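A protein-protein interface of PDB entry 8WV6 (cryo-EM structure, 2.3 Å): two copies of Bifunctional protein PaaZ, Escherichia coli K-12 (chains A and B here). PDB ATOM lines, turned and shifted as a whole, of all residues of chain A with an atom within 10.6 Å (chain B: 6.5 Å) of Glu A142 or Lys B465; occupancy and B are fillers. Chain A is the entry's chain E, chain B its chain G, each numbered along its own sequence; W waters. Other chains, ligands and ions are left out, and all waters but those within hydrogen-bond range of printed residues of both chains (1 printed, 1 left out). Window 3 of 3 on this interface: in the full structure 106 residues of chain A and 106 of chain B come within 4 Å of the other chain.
The backbone NH (N) of Gly A144 sits at hydrogen-bond distance from the side-chain hydroxyl (OG) of Ser A140. N of Glu B462 sits close to OD1 of Asn B460 (3.5 Å). The side-chain amide oxygen (OD1) of Asn B460 sits at hydrogen-bond distance from the side-chain hydroxyl (OG) of Ser B463. The backbone NH (N) of Ala A146 lies within hydrogen-bond range of the backbone carbonyl oxygen (O) of Gly A508, at 2.8 Å. The side-chain hydroxyl (OG) of Ser A140 lies within hydrogen-bond range of the backbone NH (N) of Gly A143 (3.0 Å). The side-chain hydroxyl (OG) of Ser A140 sits at hydrogen-bond distance from the backbone NH (N) of Phe A145 (3.3 Å).
No position is printed for both chains.
The side-chain carboxylate (OE1) of Glu B466 is in hydrogen-bond range of the backbone NH (N) of Glu A142, 2.7 Å away. The side-chain carboxylate of Glu B466 sits at hydrogen-bond distance from the backbone NH of Lys A141 (2.7 Å). NZ of Lys B465 is in salt-bridge range of OE1 of Glu A142 (3.2 Å).
Water W1 lies within hydrogen-bond range of the backbone NH of Ser A509, the side-chain amide oxygen of Asn B460 and the side-chain hydroxyl of Ser B463.
Of the 16 printed residues of chain A, 7 touch a printed residue of chain B. Printed residues of chain A that touch a printed residue of chain B: Ser A140, Lys A141, Glu A142, Gly A144, Phe A145, Gly A508 and Ser A509. Hydrophobic or aromatic side chains of chain A that line the printed part of chain B: Phe A145. Printed residues of chain B that touch a printed residue of chain A: Asn B460, Glu B462, Ser B463, Lys B465, Glu B466 and Ser B467. Among the printed residues, 12 pairs touch across the chains.
Of chain B, only Lys B465 and Glu B466 come within 4 Å of Glu A142. Of the printed residues of chain B, Phe A145 touches Glu B466 and Ser B467. Printed residues of chain B within 4 Å of Gly A508: Ser B463. Of the printed residues of chain A, Glu B462 touches Gly A144 (3.9999 Å) and Ser A509 (3.7 Å). Of the printed residues of chain A, Ser B463 touches Gly A144 (3.4 Å), Gly A508 (3.99 Å) and Ser A509 (3.7 Å). No residue of chain A comes within 4 Å of Ala B464. Of the printed residues of chain A, Lys B465 touches Glu A142 (3.2 Å). Glu B466 touches just these residues of chain A: Ser A140 (3.4 Å), Lys A141 (2.7 Å), Glu A142 (2.7 Å) and Phe A145 (3.9 Å). Printed residues of chain A within 4 Å of Ser B467: Phe A145. The nearest printed residue of chain B that does not touch Glu A142 is Glu B462 (6.7 Å). The nearest printed residue of chain B that does not touch Gly A144 is Glu B466 (4.6 Å).
Among the printed residues, pairs that only touch across the chains: Ser A140 with Glu B466 (3.4 Å), Gly A144 with Glu B462 (3.9999 Å), Gly A144 with Ser B463 (3.4 Å), Phe A145 with Glu B466 (3.9 Å), Phe A145 with Ser B467 (3.5 Å), Gly A508 with Ser B463 (3.99 Å), Ser A509 with Asn B460 (3.9 Å), Ser A509 with Glu B462 (3.7 Å) and Ser A509 with Ser B463 (3.7 Å).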
ATOM      1  N   LEU A 136       3.579   1.288  19.065  1.00  0.00           N
ATOM      2  CA  LEU A 136       3.794   2.706  19.314  1.00  0.00           C
ATOM      3  C   LEU A 136       4.429   2.939  20.678  1.00  0.00           C
ATOM      4  O   LEU A 136       4.028   2.333  21.673  1.00  0.00           O
ATOM      5  CB  LEU A 136       2.469   3.451  19.225  1.00  0.00           C
ATOM      6  CG  LEU A 136       2.543   4.963  19.374  1.00  0.00           C
ATOM      7  CD1 LEU A 136       2.940   5.578  18.063  1.00  0.00           C
ATOM      8  CD2 LEU A 136       1.230   5.515  19.860  1.00  0.00           C
ATOM      9  N   PRO A 138       4.889   5.659  23.500  1.00  0.00           N
ATOM     10  CA  PRO A 138       4.422   6.972  23.959  1.00  0.00           C
ATOM     11  C   PRO A 138       5.563   7.787  24.548  1.00  0.00           C
ATOM     12  O   PRO A 138       6.394   7.275  25.298  1.00  0.00           O
ATOM     13  CB  PRO A 138       3.364   6.626  25.012  1.00  0.00           C
ATOM     14  CG  PRO A 138       3.720   5.272  25.479  1.00  0.00           C
ATOM     15  CD  PRO A 138       4.427   4.564  24.368  1.00  0.00           C
ATOM     16  N   LEU A 139       5.603   9.072  24.189  1.00  0.00           N
ATOM     17  CA  LEU A 139       6.666   9.966  24.632  1.00  0.00           C
ATOM     18  C   LEU A 139       6.153  11.266  25.237  1.00  0.00           C
ATOM     19  O   LEU A 139       6.874  12.265  25.210  1.00  0.00           O
ATOM     20  CB  LEU A 139       7.614  10.302  23.474  1.00  0.00           C
ATOM     21  CG  LEU A 139       8.280   9.148  22.733  1.00  0.00           C
ATOM     22  CD1 LEU A 139       8.855   9.643  21.424  1.00  0.00           C
ATOM     23  CD2 LEU A 139       9.342   8.506  23.588  1.00  0.00           C
ATOM     24  N   SER A 140       4.937  11.295  25.775  1.00  0.00           N
ATOM     25  CA  SER A 140       4.391  12.545  26.275  1.00  0.00           C
ATOM     26  C   SER A 140       3.361  12.263  27.357  1.00  0.00           C
ATOM     27  O   SER A 140       2.941  11.122  27.564  1.00  0.00           O
ATOM     28  CB  SER A 140       3.774  13.378  25.143  1.00  0.00           C
ATOM     29  OG  SER A 140       2.604  12.779  24.627  1.00  0.00           O
ATOM     30  N   LYS A 141       2.964  13.332  28.054  1.00  0.00           N
ATOM     31  CA  LYS A 141       1.934  13.223  29.084  1.00  0.00           C
ATOM     32  C   LYS A 141       0.548  13.092  28.467  1.00  0.00           C
ATOM     33  O   LYS A 141      -0.194  12.156  28.781  1.00  0.00           O
ATOM     34  CB  LYS A 141       1.970  14.445  30.001  1.00  0.00           C
ATOM     35  CG  LYS A 141       3.268  14.690  30.751  1.00  0.00           C
ATOM     36  CD  LYS A 141       3.528  13.675  31.835  1.00  0.00           C
ATOM     37  CE  LYS A 141       4.826  13.998  32.558  1.00  0.00           C
ATOM     38  NZ  LYS A 141       4.719  15.254  33.360  1.00  0.00           N
ATOM     39  N   GLU A 142       0.174  14.036  27.604  1.00  0.00           N
ATOM     40  CA  GLU A 142      -1.186  14.091  27.087  1.00  0.00           C
ATOM     41  C   GLU A 142      -1.401  13.201  25.874  1.00  0.00           C
ATOM     42  O   GLU A 142      -2.546  13.040  25.442  1.00  0.00           O
ATOM     43  CB  GLU A 142      -1.557  15.530  26.730  1.00  0.00           C
ATOM     44  CG  GLU A 142      -2.234  16.295  27.849  1.00  0.00           C
ATOM     45  CD  GLU A 142      -1.243  16.962  28.781  1.00  0.00           C
ATOM     46  OE1 GLU A 142      -0.049  16.611  28.733  1.00  0.00           O
ATOM     47  OE2 GLU A 142      -1.654  17.852  29.550  1.00  0.00           O
ATOM     48  N   GLY A 143      -0.342  12.625  25.316  1.00  0.00           N
ATOM     49  CA  GLY A 143      -0.454  11.764  24.163  1.00  0.00           C
ATOM     50  C   GLY A 143      -0.277  12.457  22.830  1.00  0.00           C
ATOM     51  O   GLY A 143      -0.709  11.913  21.808  1.00  0.00           O
ATOM     52  N   GLY A 144       0.335  13.633  22.805  1.00  0.00           N
ATOM     53  CA  GLY A 144       0.522  14.338  21.557  1.00  0.00           C
ATOM     54  C   GLY A 144       1.779  13.999  20.799  1.00  0.00           C
ATOM     55  O   GLY A 144       1.911  14.389  19.638  1.00  0.00           O
ATOM     56  N   PHE A 145       2.705  13.271  21.415  1.00  0.00           N
ATOM     57  CA  PHE A 145       4.029  13.034  20.858  1.00  0.00           C
ATOM     58  C   PHE A 145       4.428  11.592  21.138  1.00  0.00           C
ATOM     59  O   PHE A 145       4.541  11.195  22.299  1.00  0.00           O
ATOM     60  CB  PHE A 145       5.041  14.015  21.457  1.00  0.00           C
ATOM     61  CG  PHE A 145       6.417  13.890  20.895  1.00  0.00           C
ATOM     62  CD1 PHE A 145       6.663  14.174  19.569  1.00  0.00           C
ATOM     63  CD2 PHE A 145       7.469  13.496  21.696  1.00  0.00           C
ATOM     64  CE1 PHE A 145       7.929  14.067  19.056  1.00  0.00           C
ATOM     65  CE2 PHE A 145       8.738  13.380  21.181  1.00  0.00           C
ATOM     66  CZ  PHE A 145       8.966  13.666  19.855  1.00  0.00           C
ATOM     67  N   ALA A 146       4.632  10.812  20.077  1.00  0.00           N
ATOM     68  CA  ALA A 146       4.933   9.392  20.189  1.00  0.00           C
ATOM     69  C   ALA A 146       5.986   9.029  19.148  1.00  0.00           C
ATOM     70  O   ALA A 146       6.502   9.892  18.438  1.00  0.00           O
ATOM     71  CB  ALA A 146       3.663   8.554  20.026  1.00  0.00           C
ATOM     72  N   GLY A 508       6.330  11.926  16.150  1.00  0.00           N
ATOM     73  CA  GLY A 508       5.290  12.847  15.752  1.00  0.00           C
ATOM     74  C   GLY A 508       4.027  12.560  16.534  1.00  0.00           C
ATOM     75  O   GLY A 508       4.029  11.791  17.490  1.00  0.00           O
ATOM     76  N   SER A 509       2.949  13.190  16.101  1.00  0.00           N
ATOM     77  CA  SER A 509       1.677  12.943  16.741  1.00  0.00           C
ATOM     78  C   SER A 509       1.139  11.585  16.296  1.00  0.00           C
ATOM     79  O   SER A 509       1.478  11.103  15.213  1.00  0.00           O
ATOM     80  CB  SER A 509       0.681  14.048  16.414  1.00  0.00           C
ATOM     81  OG  SER A 509       0.260  13.982  15.070  1.00  0.00           O
ATOM     82  N   PRO A 510       0.334  10.931  17.134  1.00  0.00           N
ATOM     83  CA  PRO A 510      -0.229   9.634  16.732  1.00  0.00           C
ATOM     84  C   PRO A 510      -0.962   9.660  15.404  1.00  0.00           C
ATOM     85  O   PRO A 510      -0.936   8.667  14.679  1.00  0.00           O
ATOM     86  CB  PRO A 510      -1.163   9.301  17.897  1.00  0.00           C
ATOM     87  CG  PRO A 510      -0.498   9.908  19.060  1.00  0.00           C
ATOM     88  CD  PRO A 510       0.159  11.174  18.574  1.00  0.00           C
ATOM     89  N   ARG A 522      -2.727   4.012  18.833  1.00  0.00           N
ATOM     90  CA  ARG A 522      -3.462   4.553  19.967  1.00  0.00           C
ATOM     91  C   ARG A 522      -3.317   6.070  20.023  1.00  0.00           C
ATOM     92  O   ARG A 522      -2.206   6.601  19.978  1.00  0.00           O
ATOM     93  CB  ARG A 522      -2.958   3.913  21.259  1.00  0.00           C
ATOM     94  CG  ARG A 522      -3.536   4.502  22.531  1.00  0.00           C
ATOM     95  CD  ARG A 522      -4.245   3.463  23.387  1.00  0.00           C
ATOM     96  NE  ARG A 522      -3.517   2.201  23.493  1.00  0.00           N
ATOM     97  CZ  ARG A 522      -3.967   1.035  23.036  1.00  0.00           C
ATOM     98  NH1 ARG A 522      -5.149   0.966  22.440  1.00  0.00           N
ATOM     99  NH2 ARG A 522      -3.237  -0.062  23.181  1.00  0.00           N
ATOM    100  N   GLY A 523      -4.445   6.765  20.125  1.00  0.00           N
ATOM    101  CA  GLY A 523      -4.450   8.208  20.162  1.00  0.00           C
ATOM    102  C   GLY A 523      -4.736   8.887  18.841  1.00  0.00           C
ATOM    103  O   GLY A 523      -4.909  10.108  18.819  1.00  0.00           O
ATOM    104  N   ALA A 524      -4.807   8.140  17.748  1.00  0.00           N
ATOM    105  CA  ALA A 524      -4.960   8.730  16.432  1.00  0.00           C
ATOM    106  C   ALA A 524      -6.428   8.993  16.107  1.00  0.00           C
ATOM    107  O   ALA A 524      -7.342   8.382  16.666  1.00  0.00           O
ATOM    108  CB  ALA A 524      -4.336   7.823  15.372  1.00  0.00           C
ATOM    109  N   ASN B 460       4.215  19.071  13.583  1.00  0.00           N
ATOM    110  CA  ASN B 460       3.011  19.858  13.348  1.00  0.00           C
ATOM    111  C   ASN B 460       2.602  20.493  14.671  1.00  0.00           C
ATOM    112  O   ASN B 460       3.319  20.401  15.671  1.00  0.00           O
ATOM    113  CB  ASN B 460       1.898  19.000  12.723  1.00  0.00           C
ATOM    114  CG  ASN B 460       1.316  17.979  13.682  1.00  0.00           C
ATOM    115  OD1 ASN B 460       1.934  17.615  14.674  1.00  0.00           O
ATOM    116  ND2 ASN B 460       0.122  17.500  13.372  1.00  0.00           N
ATOM    117  N   GLU B 461       1.438  21.141  14.672  1.00  0.00           N
ATOM    118  CA  GLU B 461       1.004  21.893  15.845  1.00  0.00           C
ATOM    119  C   GLU B 461       0.763  20.982  17.043  1.00  0.00           C
ATOM    120  O   GLU B 461       1.077  21.351  18.180  1.00  0.00           O
ATOM    121  CB  GLU B 461      -0.258  22.685  15.511  1.00  0.00           C
ATOM    122  CG  GLU B 461      -0.607  23.770  16.506  1.00  0.00           C
ATOM    123  CD  GLU B 461      -1.874  24.522  16.121  1.00  0.00           C
ATOM    124  OE1 GLU B 461      -2.338  24.360  14.973  1.00  0.00           O
ATOM    125  OE2 GLU B 461      -2.407  25.270  16.968  1.00  0.00           O
ATOM    126  N   GLU B 462       0.223  19.785  16.811  1.00  0.00           N
ATOM    127  CA  GLU B 462      -0.137  18.917  17.929  1.00  0.00           C
ATOM    128  C   GLU B 462       1.094  18.341  18.619  1.00  0.00           C
ATOM    129  O   GLU B 462       1.160  18.312  19.851  1.00  0.00           O
ATOM    130  CB  GLU B 462      -1.058  17.792  17.459  1.00  0.00           C
ATOM    131  CG  GLU B 462      -1.236  16.711  18.511  1.00  0.00           C
ATOM    132  CD  GLU B 462      -2.243  15.650  18.123  1.00  0.00           C
ATOM    133  OE1 GLU B 462      -2.761  15.695  16.990  1.00  0.00           O
ATOM    134  OE2 GLU B 462      -2.513  14.765  18.962  1.00  0.00           O
ATOM    135  N   SER B 463       2.083  17.883  17.851  1.00  0.00           N
ATOM    136  CA  SER B 463       3.255  17.275  18.469  1.00  0.00           C
ATOM    137  C   SER B 463       4.166  18.315  19.107  1.00  0.00           C
ATOM    138  O   SER B 463       4.987  17.972  19.958  1.00  0.00           O
ATOM    139  CB  SER B 463       4.021  16.442  17.439  1.00  0.00           C
ATOM    140  OG  SER B 463       4.496  17.249  16.382  1.00  0.00           O
ATOM    141  N   ALA B 464       4.020  19.585  18.736  1.00  0.00           N
ATOM    142  CA  ALA B 464       4.950  20.613  19.188  1.00  0.00           C
ATOM    143  C   ALA B 464       4.825  20.946  20.668  1.00  0.00           C
ATOM    144  O   ALA B 464       5.747  21.559  21.214  1.00  0.00           O
ATOM    145  CB  ALA B 464       4.764  21.887  18.369  1.00  0.00           C
ATOM    146  N   LYS B 465       3.733  20.566  21.333  1.00  0.00           N
ATOM    147  CA  LYS B 465       3.525  21.012  22.709  1.00  0.00           C
ATOM    148  C   LYS B 465       4.306  20.151  23.699  1.00  0.00           C
ATOM    149  O   LYS B 465       4.619  20.596  24.808  1.00  0.00           O
ATOM    150  CB  LYS B 465       2.030  21.018  23.038  1.00  0.00           C
ATOM    151  CG  LYS B 465       1.677  21.597  24.411  1.00  0.00           C
ATOM    152  CD  LYS B 465       1.461  20.555  25.502  1.00  0.00           C
ATOM    153  CE  LYS B 465       0.141  19.828  25.327  1.00  0.00           C
ATOM    154  NZ  LYS B 465      -0.089  18.835  26.414  1.00  0.00           N
ATOM    155  N   GLU B 466       4.632  18.912  23.318  1.00  0.00           N
ATOM    156  CA  GLU B 466       5.377  18.011  24.192  1.00  0.00           C
ATOM    157  C   GLU B 466       6.571  17.384  23.482  1.00  0.00           C
ATOM    158  O   GLU B 466       7.275  16.558  24.066  1.00  0.00           O
ATOM    159  CB  GLU B 466       4.475  16.917  24.761  1.00  0.00           C
ATOM    160  CG  GLU B 466       3.348  17.420  25.649  1.00  0.00           C
ATOM    161  CD  GLU B 466       2.862  16.365  26.617  1.00  0.00           C
ATOM    162  OE1 GLU B 466       1.672  16.009  26.550  1.00  0.00           O
ATOM    163  OE2 GLU B 466       3.666  15.898  27.451  1.00  0.00           O
ATOM    164  N   SER B 467       6.811  17.762  22.227  1.00  0.00           N
ATOM    165  CA  SER B 467       7.931  17.213  21.473  1.00  0.00           C
ATOM    166  C   SER B 467       9.244  17.423  22.213  1.00  0.00           C
ATOM    167  O   SER B 467       9.438  18.438  22.886  1.00  0.00           O
ATOM    168  CB  SER B 467       8.004  17.859  20.092  1.00  0.00           C
ATOM    169  OG  SER B 467       9.096  17.350  19.358  1.00  0.00           O
HETATM  170  O   HOH W   1       3.101  15.174  14.243  1.00  0.00           O
